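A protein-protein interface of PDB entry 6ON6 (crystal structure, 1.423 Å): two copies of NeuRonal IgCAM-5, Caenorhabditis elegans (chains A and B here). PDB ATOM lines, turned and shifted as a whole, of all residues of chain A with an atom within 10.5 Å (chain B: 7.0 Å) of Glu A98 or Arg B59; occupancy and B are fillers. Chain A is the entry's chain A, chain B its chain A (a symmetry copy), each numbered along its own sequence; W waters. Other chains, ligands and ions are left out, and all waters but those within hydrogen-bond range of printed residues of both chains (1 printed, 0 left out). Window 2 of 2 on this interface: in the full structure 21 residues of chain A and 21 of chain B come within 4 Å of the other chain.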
ATOM      1  N   ALA A   4       3.513  -7.333  10.319  1.00  0.00           N
ATOM      2  CA  ALA A   4       2.591  -7.294  11.446  1.00  0.00           C
ATOM      3  C   ALA A   4       1.330  -6.572  11.043  1.00  0.00           C
ATOM      4  O   ALA A   4       1.399  -5.566  10.338  1.00  0.00           O
ATOM      5  CB  ALA A   4       3.221  -6.592  12.627  1.00  0.00           C
ATOM      6  N   PRO A   5       0.189  -7.088  11.490  1.00  0.00           N
ATOM      7  CA  PRO A   5      -1.078  -6.394  11.290  1.00  0.00           C
ATOM      8  C   PRO A   5      -1.180  -5.224  12.252  1.00  0.00           C
ATOM      9  O   PRO A   5      -0.437  -5.157  13.238  1.00  0.00           O
ATOM     10  CB  PRO A   5      -2.109  -7.477  11.643  1.00  0.00           C
ATOM     11  CG  PRO A   5      -1.418  -8.310  12.670  1.00  0.00           C
ATOM     12  CD  PRO A   5       0.018  -8.346  12.241  1.00  0.00           C
ATOM     13  N   PRO A   6      -2.071  -4.270  12.008  1.00  0.00           N
ATOM     14  CA  PRO A   6      -2.309  -3.250  13.031  1.00  0.00           C
ATOM     15  C   PRO A   6      -2.787  -3.882  14.323  1.00  0.00           C
ATOM     16  O   PRO A   6      -3.598  -4.815  14.318  1.00  0.00           O
ATOM     17  CB  PRO A   6      -3.417  -2.380  12.414  1.00  0.00           C
ATOM     18  CG  PRO A   6      -3.200  -2.516  10.938  1.00  0.00           C
ATOM     19  CD  PRO A   6      -2.672  -3.933  10.712  1.00  0.00           C
ATOM     20  N   THR A   7      -2.339  -3.308  15.443  1.00  0.00           N
ATOM     21  CA  THR A   7      -2.846  -3.688  16.747  1.00  0.00           C
ATOM     22  C   THR A   7      -3.072  -2.408  17.545  1.00  0.00           C
ATOM     23  O   THR A   7      -2.458  -1.373  17.290  1.00  0.00           O
ATOM     24  CB  THR A   7      -1.873  -4.662  17.469  1.00  0.00           C
ATOM     25  OG1 THR A   7      -0.563  -4.083  17.476  1.00  0.00           O
ATOM     26  CG2 THR A   7      -1.862  -6.041  16.783  1.00  0.00           C
ATOM     27  N   ASP A  32       1.705  -0.504  14.127  1.00  0.00           N
ATOM     28  CA  ASP A  32       1.733  -1.139  12.806  1.00  0.00           C
ATOM     29  C   ASP A  32       0.501  -0.801  11.955  1.00  0.00           C
ATOM     30  O   ASP A  32      -0.092  -1.661  11.303  1.00  0.00           O
ATOM     31  CB  ASP A  32       1.964  -2.648  12.932  1.00  0.00           C
ATOM     32  CG  ASP A  32       3.247  -2.964  13.687  1.00  0.00           C
ATOM     33  OD1 ASP A  32       4.312  -2.473  13.263  1.00  0.00           O
ATOM     34  OD2 ASP A  32       3.169  -3.648  14.725  1.00  0.00           O
ATOM     35  N   LEU A  33       0.076   0.471  11.997  1.00  0.00           N
ATOM     36  CA  LEU A  33      -1.106   0.875  11.235  1.00  0.00           C
ATOM     37  C   LEU A  33      -0.887   0.726   9.733  1.00  0.00           C
ATOM     38  O   LEU A  33      -1.803   0.323   9.007  1.00  0.00           O
ATOM     39  CB  LEU A  33      -1.498   2.316  11.582  1.00  0.00           C
ATOM     40  CG  LEU A  33      -2.743   2.804  10.846  1.00  0.00           C
ATOM     41  CD1 LEU A  33      -3.974   2.067  11.346  1.00  0.00           C
ATOM     42  CD2 LEU A  33      -2.903   4.307  11.014  1.00  0.00           C
ATOM     43  N   HIS A  36      -3.579   1.483   6.748  1.00  0.00           N
ATOM     44  CA  HIS A  36      -4.948   1.305   7.175  1.00  0.00           C
ATOM     45  C   HIS A  36      -5.539   2.611   7.696  1.00  0.00           C
ATOM     46  O   HIS A  36      -4.829   3.562   8.034  1.00  0.00           O
ATOM     47  CB  HIS A  36      -5.031   0.194   8.206  1.00  0.00           C
ATOM     48  CG  HIS A  36      -4.862  -1.168   7.618  1.00  0.00           C
ATOM     49  ND1 HIS A  36      -3.640  -1.806   7.543  1.00  0.00           N
ATOM     50  CD2 HIS A  36      -5.764  -2.011   7.064  1.00  0.00           C
ATOM     51  CE1 HIS A  36      -3.805  -2.986   6.976  1.00  0.00           C
ATOM     52  NE2 HIS A  36      -5.081  -3.139   6.681  1.00  0.00           N
ATOM     53  N   MET A  37      -6.863   2.657   7.713  1.00  0.00           N
ATOM     54  CA  MET A  37      -7.621   3.836   8.130  1.00  0.00           C
ATOM     55  C   MET A  37      -8.189   3.638   9.526  1.00  0.00           C
ATOM     56  O   MET A  37      -8.658   2.546   9.861  1.00  0.00           O
ATOM     57  CB  MET A  37      -8.789   4.042   7.166  1.00  0.00           C
ATOM     58  CG  MET A  37      -8.369   4.393   5.772  1.00  0.00           C
ATOM     59  SD  MET A  37      -7.799   6.094   5.678  1.00  0.00           S
ATOM     60  CE  MET A  37      -6.029   5.879   5.699  1.00  0.00           C
ATOM     61  N   GLN A  94     -11.842   2.150  15.367  1.00  0.00           N
ATOM     62  CA  GLN A  94     -11.823   0.947  14.554  1.00  0.00           C
ATOM     63  C   GLN A  94     -10.915   1.147  13.355  1.00  0.00           C
ATOM     64  O   GLN A  94     -10.817   2.256  12.821  1.00  0.00           O
ATOM     65  CB  GLN A  94     -13.238   0.508  14.229  1.00  0.00           C
ATOM     66  CG  GLN A  94     -13.963   1.392  13.357  1.00  0.00           C
ATOM     67  CD  GLN A  94     -15.447   0.997  13.287  1.00  0.00           C
ATOM     68  OE1 GLN A  94     -16.167   1.037  14.291  1.00  0.00           O
ATOM     69  NE2 GLN A  94     -15.877   0.551  12.130  1.00  0.00           N
ATOM     70  N   ILE A  95     -10.153   0.084  13.012  1.00  0.00           N
ATOM     71  CA  ILE A  95      -9.217   0.116  11.903  1.00  0.00           C
ATOM     72  C   ILE A  95      -9.687  -0.870  10.860  1.00  0.00           C
ATOM     73  O   ILE A  95     -10.211  -1.928  11.216  1.00  0.00           O
ATOM     74  CB  ILE A  95      -7.838  -0.338  12.401  1.00  0.00           C
ATOM     75  CG1 ILE A  95      -7.498   0.368  13.723  1.00  0.00           C
ATOM     76  CG2 ILE A  95      -6.819  -0.013  11.364  1.00  0.00           C
ATOM     77  CD1 ILE A  95      -6.363  -0.291  14.504  1.00  0.00           C
ATOM     78  N   ASN A  96      -9.575  -0.488   9.578  1.00  0.00           N
ATOM     79  CA  ASN A  96     -10.109  -1.298   8.472  1.00  0.00           C
ATOM     80  C   ASN A  96      -9.247  -2.486   8.099  1.00  0.00           C
ATOM     81  O   ASN A  96      -9.030  -2.752   6.914  1.00  0.00           O
ATOM     82  CB  ASN A  96     -10.405  -0.470   7.226  1.00  0.00           C
ATOM     83  CG  ASN A  96      -9.186   0.176   6.664  1.00  0.00           C
ATOM     84  OD1 ASN A  96      -8.119   0.173   7.295  1.00  0.00           O
ATOM     85  ND2 ASN A  96      -9.312   0.726   5.464  1.00  0.00           N
ATOM     86  N   THR A  97      -8.798  -3.201   9.106  1.00  0.00           N
ATOM     87  CA  THR A  97      -8.135  -4.467   8.862  1.00  0.00           C
ATOM     88  C   THR A  97      -9.167  -5.550   8.622  1.00  0.00           C
ATOM     89  O   THR A  97     -10.376  -5.391   8.855  1.00  0.00           O
ATOM     90  CB  THR A  97      -7.313  -4.830  10.080  1.00  0.00           C
ATOM     91  OG1 THR A  97      -8.138  -4.779  11.257  1.00  0.00           O
ATOM     92  CG2 THR A  97      -6.134  -3.885  10.215  1.00  0.00           C
ATOM     93  N   GLU A  98      -8.656  -6.665   8.114  1.00  0.00           N
ATOM     94  CA  GLU A  98      -9.420  -7.886   7.924  1.00  0.00           C
ATOM     95  C   GLU A  98      -8.611  -8.953   8.641  1.00  0.00           C
ATOM     96  O   GLU A  98      -7.516  -9.331   8.168  1.00  0.00           O
ATOM     97  CB  GLU A  98      -9.598  -8.214   6.441  1.00  0.00           C
ATOM     98  CG  GLU A  98     -10.552  -7.222   5.797  1.00  0.00           C
ATOM     99  CD  GLU A  98     -10.459  -7.127   4.289  1.00  0.00           C
ATOM    100  OE1 GLU A  98      -9.867  -8.054   3.660  1.00  0.00           O
ATOM    101  OE2 GLU A  98     -10.985  -6.102   3.757  1.00  0.00           O
ATOM    102  N   PRO A  99      -9.085  -9.449   9.776  1.00  0.00           N
ATOM    103  CA  PRO A  99     -10.330  -8.957  10.377  1.00  0.00           C
ATOM    104  C   PRO A  99     -10.173  -7.593  11.077  1.00  0.00           C
ATOM    105  O   PRO A  99      -9.065  -7.069  11.212  1.00  0.00           O
ATOM    106  CB  PRO A  99     -10.648 -10.021  11.415  1.00  0.00           C
ATOM    107  CG  PRO A  99      -9.286 -10.532  11.833  1.00  0.00           C
ATOM    108  CD  PRO A  99      -8.439 -10.504  10.573  1.00  0.00           C
ATOM    109  N   ILE A 100     -11.282  -7.052  11.557  1.00  0.00           N
ATOM    110  CA  ILE A 100     -11.254  -5.678  12.068  1.00  0.00           C
ATOM    111  C   ILE A 100     -10.435  -5.606  13.347  1.00  0.00           C
ATOM    112  O   ILE A 100     -10.216  -6.584  14.052  1.00  0.00           O
ATOM    113  CB  ILE A 100     -12.694  -5.208  12.304  1.00  0.00           C
ATOM    114  CG1 ILE A 100     -12.770  -3.689  12.430  1.00  0.00           C
ATOM    115  CG2 ILE A 100     -13.241  -5.950  13.526  1.00  0.00           C
ATOM    116  CD1 ILE A 100     -14.113  -3.197  12.232  1.00  0.00           C
ATOM    117  N   THR A 101      -9.988  -4.411  13.654  1.00  0.00           N
ATOM    118  CA  THR A 101      -9.304  -4.165  14.908  1.00  0.00           C
ATOM    119  C   THR A 101     -10.003  -2.976  15.547  1.00  0.00           C
ATOM    120  O   THR A 101     -10.248  -1.970  14.866  1.00  0.00           O
ATOM    121  CB  THR A 101      -7.855  -3.842  14.622  1.00  0.00           C
ATOM    122  OG1 THR A 101      -7.281  -4.934  13.881  1.00  0.00           O
ATOM    123  CG2 THR A 101      -7.113  -3.683  15.909  1.00  0.00           C
ATOM    124  N   LEU A 102     -10.383  -3.131  16.807  1.00  0.00           N
ATOM    125  CA  LEU A 102     -11.111  -2.052  17.466  1.00  0.00           C
ATOM    126  C   LEU A 102     -10.938  -2.110  18.974  1.00  0.00           C
ATOM    127  O   LEU A 102     -10.474  -3.103  19.547  1.00  0.00           O
ATOM    128  CB  LEU A 102     -12.582  -2.093  17.088  1.00  0.00           C
ATOM    129  CG  LEU A 102     -13.486  -3.236  17.514  1.00  0.00           C
ATOM    130  CD1 LEU A 102     -14.076  -2.967  18.882  1.00  0.00           C
ATOM    131  CD2 LEU A 102     -14.588  -3.339  16.483  1.00  0.00           C
ATOM    132  N   ARG B  48     -20.300  -0.541  13.050  1.00  0.00           N
ATOM    133  CA  ARG B  48     -19.290  -0.779  12.034  1.00  0.00           C
ATOM    134  C   ARG B  48     -19.457   0.267  10.956  1.00  0.00           C
ATOM    135  O   ARG B  48     -20.530   0.369  10.355  1.00  0.00           O
ATOM    136  CB  ARG B  48     -19.495  -2.147  11.424  1.00  0.00           C
ATOM    137  CG  ARG B  48     -19.232  -3.271  12.409  1.00  0.00           C
ATOM    138  CD  ARG B  48     -17.828  -3.218  12.960  1.00  0.00           C
ATOM    139  NE  ARG B  48     -17.548  -4.415  13.747  1.00  0.00           N
ATOM    140  CZ  ARG B  48     -17.162  -5.579  13.224  1.00  0.00           C
ATOM    141  NH1 ARG B  48     -16.999  -5.702  11.908  1.00  0.00           N
ATOM    142  NH2 ARG B  48     -16.936  -6.621  14.014  1.00  0.00           N
ATOM    143  N   VAL B  56     -15.618   1.818   0.093  1.00  0.00           N
ATOM    144  CA  VAL B  56     -15.902   0.897   1.187  1.00  0.00           C
ATOM    145  C   VAL B  56     -14.749   0.918   2.191  1.00  0.00           C
ATOM    146  O   VAL B  56     -13.570   1.026   1.824  1.00  0.00           O
ATOM    147  CB  VAL B  56     -16.175  -0.498   0.603  1.00  0.00           C
ATOM    148  CG1 VAL B  56     -16.324  -1.512   1.649  1.00  0.00           C
ATOM    149  CG2 VAL B  56     -17.421  -0.471  -0.206  1.00  0.00           C
ATOM    150  N   PHE B  57     -15.088   0.801   3.470  1.00  0.00           N
ATOM    151  CA  PHE B  57     -14.071   0.827   4.522  1.00  0.00           C
ATOM    152  C   PHE B  57     -13.167  -0.396   4.430  1.00  0.00           C
ATOM    153  O   PHE B  57     -11.939  -0.282   4.490  1.00  0.00           O
ATOM    154  CB  PHE B  57     -14.785   0.892   5.876  1.00  0.00           C
ATOM    155  CG  PHE B  57     -13.896   1.190   7.052  1.00  0.00           C
ATOM    156  CD1 PHE B  57     -13.009   2.268   7.040  1.00  0.00           C
ATOM    157  CD2 PHE B  57     -14.054   0.474   8.223  1.00  0.00           C
ATOM    158  CE1 PHE B  57     -12.243   2.585   8.166  1.00  0.00           C
ATOM    159  CE2 PHE B  57     -13.277   0.774   9.369  1.00  0.00           C
ATOM    160  CZ  PHE B  57     -12.381   1.839   9.337  1.00  0.00           C
ATOM    161  N   ARG B  58     -13.758  -1.566   4.261  1.00  0.00           N
ATOM    162  CA  ARG B  58     -13.030  -2.829   4.259  1.00  0.00           C
ATOM    163  C   ARG B  58     -13.946  -3.874   3.655  1.00  0.00           C
ATOM    164  O   ARG B  58     -15.128  -3.607   3.417  1.00  0.00           O
ATOM    165  CB  ARG B  58     -12.694  -3.219   5.688  1.00  0.00           C
ATOM    166  CG  ARG B  58     -13.901  -3.100   6.599  1.00  0.00           C
ATOM    167  CD  ARG B  58     -13.539  -3.221   8.061  1.00  0.00           C
ATOM    168  NE  ARG B  58     -13.001  -4.534   8.361  1.00  0.00           N
ATOM    169  CZ  ARG B  58     -13.737  -5.591   8.692  1.00  0.00           C
ATOM    170  NH1 ARG B  58     -13.127  -6.735   8.938  1.00  0.00           N
ATOM    171  NH2 ARG B  58     -15.062  -5.490   8.813  1.00  0.00           N
ATOM    172  N   ARG B  59     -13.399  -5.077   3.457  1.00  0.00           N
ATOM    173  CA  ARG B  59     -14.121  -6.238   2.917  1.00  0.00           C
ATOM    174  C   ARG B  59     -14.828  -5.892   1.602  1.00  0.00           C
ATOM    175  O   ARG B  59     -16.052  -5.985   1.474  1.00  0.00           O
ATOM    176  CB  ARG B  59     -15.113  -6.838   3.929  1.00  0.00           C
ATOM    177  CG  ARG B  59     -14.486  -7.318   5.206  1.00  0.00           C
ATOM    178  CD  ARG B  59     -15.558  -7.927   6.115  1.00  0.00           C
ATOM    179  NE  ARG B  59     -16.123  -9.163   5.582  1.00  0.00           N
ATOM    180  CZ  ARG B  59     -17.219  -9.779   6.039  1.00  0.00           C
ATOM    181  NH1 ARG B  59     -17.914  -9.258   7.042  1.00  0.00           N
ATOM    182  NH2 ARG B  59     -17.612 -10.939   5.493  1.00  0.00           N
ATOM    183  N   ARG B  60     -13.996  -5.595   0.602  1.00  0.00           N
ATOM    184  CA  ARG B  60     -14.474  -5.237  -0.732  1.00  0.00           C
ATOM    185  C   ARG B  60     -15.219  -6.384  -1.424  1.00  0.00           C
ATOM    186  O   ARG B  60     -16.003  -6.132  -2.354  1.00  0.00           O
ATOM    187  CB  ARG B  60     -13.269  -4.815  -1.585  1.00  0.00           C
ATOM    188  CG  ARG B  60     -13.235  -3.354  -1.975  1.00  0.00           C
ATOM    189  N   ASN B  61     -14.976  -7.637  -1.019  1.00  0.00           N
ATOM    190  CA  ASN B  61     -15.748  -8.751  -1.565  1.00  0.00           C
ATOM    191  C   ASN B  61     -17.087  -8.945  -0.865  1.00  0.00           C
ATOM    192  O   ASN B  61     -17.909  -9.744  -1.344  1.00  0.00           O
ATOM    193  CB  ASN B  61     -14.941 -10.054  -1.512  1.00  0.00           C
ATOM    194  CG  ASN B  61     -13.732 -10.015  -2.414  1.00  0.00           C
ATOM    195  OD1 ASN B  61     -13.773  -9.410  -3.489  1.00  0.00           O
ATOM    196  ND2 ASN B  61     -12.642 -10.648  -1.980  1.00  0.00           N
ATOM    197  N   LYS B  62     -17.315  -8.270   0.259  1.00  0.00           N
ATOM    198  CA  LYS B  62     -18.555  -8.396   1.025  1.00  0.00           C
ATOM    199  C   LYS B  62     -19.520  -7.223   0.823  1.00  0.00           C
ATOM    200  O   LYS B  62     -20.732  -7.413   0.713  1.00  0.00           O
ATOM    201  CB  LYS B  62     -18.203  -8.463   2.511  1.00  0.00           C
ATOM    202  CG  LYS B  62     -19.443  -8.523   3.434  1.00  0.00           C
ATOM    203  CD  LYS B  62     -20.265  -9.805   3.184  1.00  0.00           C
ATOM    204  CE  LYS B  62     -21.441  -9.888   4.195  1.00  0.00           C
ATOM    205  NZ  LYS B  62     -22.183 -11.200   4.105  1.00  0.00           N
ATOM    206  N   TYR B  63     -18.999  -6.018   0.797  1.00  0.00           N
ATOM    207  CA  TYR B  63     -19.776  -4.802   0.645  1.00  0.00           C
ATOM    208  C   TYR B  63     -19.279  -4.154  -0.618  1.00  0.00           C
ATOM    209  O   TYR B  63     -18.062  -4.108  -0.879  1.00  0.00           O
ATOM    210  CB  TYR B  63     -19.439  -3.867   1.756  1.00  0.00           C
ATOM    211  CG  TYR B  63     -19.802  -4.408   3.086  1.00  0.00           C
ATOM    212  CD1 TYR B  63     -21.129  -4.549   3.453  1.00  0.00           C
ATOM    213  CD2 TYR B  63     -18.823  -4.817   3.964  1.00  0.00           C
ATOM    214  CE1 TYR B  63     -21.468  -5.075   4.673  1.00  0.00           C
ATOM    215  CE2 TYR B  63     -19.141  -5.318   5.175  1.00  0.00           C
ATOM    216  CZ  TYR B  63     -20.461  -5.441   5.539  1.00  0.00           C
ATOM    217  OH  TYR B  63     -20.749  -5.966   6.763  1.00  0.00           O
ATOM    218  N   GLU B  64     -20.220  -3.663  -1.395  1.00  0.00           N
ATOM    219  CA  GLU B  64     -19.889  -2.905  -2.570  1.00  0.00           C
ATOM    220  C   GLU B  64     -20.587  -1.574  -2.435  1.00  0.00           C
ATOM    221  O   GLU B  64     -21.678  -1.472  -1.871  1.00  0.00           O
ATOM    222  CB  GLU B  64     -20.314  -3.624  -3.859  1.00  0.00           C
ATOM    223  CG  GLU B  64     -19.730  -5.019  -4.005  1.00  0.00           C
ATOM    224  CD  GLU B  64     -20.056  -5.650  -5.342  1.00  0.00           C
ATOM    225  OE1 GLU B  64     -20.855  -5.046  -6.090  1.00  0.00           O
ATOM    226  OE2 GLU B  64     -19.497  -6.734  -5.652  1.00  0.00           O
ATOM    227  N   LYS B  81     -23.357  -8.403   0.015  1.00  0.00           N
ATOM    228  CA  LYS B  81     -23.322  -9.644  -0.737  1.00  0.00           C
ATOM    229  C   LYS B  81     -23.459 -10.826   0.209  1.00  0.00           C
ATOM    230  O   LYS B  81     -22.976 -10.792   1.348  1.00  0.00           O
ATOM    231  CB  LYS B  81     -21.977  -9.758  -1.460  1.00  0.00           C
ATOM    232  CG  LYS B  81     -21.707  -8.622  -2.490  1.00  0.00           C
ATOM    233  CD  LYS B  81     -22.511  -8.839  -3.737  1.00  0.00           C
ATOM    234  CE  LYS B  81     -21.861  -9.987  -4.533  1.00  0.00           C
ATOM    235  NZ  LYS B  81     -22.576 -10.335  -5.809  1.00  0.00           N
ATOM    236  N   SER B  86     -25.317 -12.966  10.543  1.00  0.00           N
ATOM    237  CA  SER B  86     -24.592 -11.869  11.160  1.00  0.00           C
ATOM    238  C   SER B  86     -24.858 -10.534  10.471  1.00  0.00           C
ATOM    239  O   SER B  86     -24.556  -9.492  11.061  1.00  0.00           O
ATOM    240  CB  SER B  86     -23.091 -12.134  11.183  1.00  0.00           C
ATOM    241  OG  SER B  86     -22.666 -12.512   9.902  1.00  0.00           O
ATOM    242  N   ASP B  87     -25.419 -10.540   9.252  1.00  0.00           N
ATOM    243  CA  ASP B  87     -25.779  -9.288   8.582  1.00  0.00           C
ATOM    244  C   ASP B  87     -27.117  -8.724   9.019  1.00  0.00           C
ATOM    245  O   ASP B  87     -27.437  -7.592   8.615  1.00  0.00           O
ATOM    246  CB  ASP B  87     -25.793  -9.525   7.073  1.00  0.00           C
ATOM    247  CG  ASP B  87     -24.431  -9.937   6.546  1.00  0.00           C
ATOM    248  OD1 ASP B  87     -23.448  -9.264   6.899  1.00  0.00           O
ATOM    249  OD2 ASP B  87     -24.354 -10.909   5.793  1.00  0.00           O
HETATM  250  O   HOH W   1     -11.286  -5.801   1.064  1.00  0.00           O
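The backbone carbonyl oxygen (O) of Phe B57 is in hydrogen-bond range of the side-chain amide nitrogen (ND2) of Asn A96. O of Thr A97 is in hydrogen-bond range of NE of Arg B58 (2.8 Å). OE2 of Glu A98 is in hydrogen-bond range of N of Arg B59, at 2.6 Å. The backbone NH (N) of Ile A100 sits close to the guanidinium group (NH1) of Arg B58 (3.2 Å).
N of Met A37 is in hydrogen-bond range of OD1 of Asn A96 (2.8 Å). The backbone carbonyl oxygen of Pro A99 sits at hydrogen-bond distance from the side-chain hydroxyl of Thr A97, 2.5 Å away. OG1 of Thr A101 is in hydrogen-bond range of OG1 of Thr A97, at 2.8 Å.
Among the printed residues, merely in contact across the chains: Met A37 with Phe B57 (3.8 Å), Gln A94 with Arg B48 (3.7 Å), Gln A94 with Phe B57 (3.8 Å), Asn A96 with Arg B58 (3.9 Å), Glu A98 with Arg B58 (3.7 Å), Pro A99 with Arg B58 (3.7 Å) and Ile A100 with Arg B48 (3.8 Å).
Printed residues of chain B within 4 Å of Asn A96: Phe B57 and Arg B58. Printed residues of chain B within 4 Å of Thr A97: Arg B58 (2.8 Å). Printed residues of chain B within 4 Å of Pro A99: Arg B58 (3.7 Å). Of the printed residues of chain A, Arg B48 touches Gln A94 (3.7 Å) and Ile A100 (3.8 Å). Printed residues of chain A within 4 Å of Phe B57: Met A37 (3.8 Å), Gln A94 (3.8 Å) and Asn A96 (3.0 Å). Arg B58 touches just these residues of chain A: Asn A96 (3.9 Å), Thr A97 (2.8 Å), Glu A98 (3.7 Å), Pro A99 (3.7 Å) and Ile A100 (3.2 Å). Arg B59 touches just one residue of chain A: Glu A98. No residue of chain A comes within 4 Å of Arg B60. No residue of chain A comes within 4 Å of Asn B61. No residue of chain A comes within 4 Å of Lys B62. No residue of chain A comes within 4 Å of Tyr B63. The nearest printed residue of chain A that does not touch Arg B48 is Leu A102 (4.2 Å).
Hydrophobic or aromatic side chains of chain B within 4 Å of the printed part of chain A: Phe B57. Along chain B the printed residues that touch a printed residue of chain A span positions 48 to 59.
No position is printed for both chains. Of the 11 pairs that touch across the chains among the printed residues, none has its exchanged pair printed and touching as well.
Water W1 lies within hydrogen-bond range of the side-chain carboxylate (OE2) of Glu A98 (2.7 Å), the backbone NH (N) of Arg B60 (2.8 Å) and the backbone NH (N) of Arg B59 (3.3 Å).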
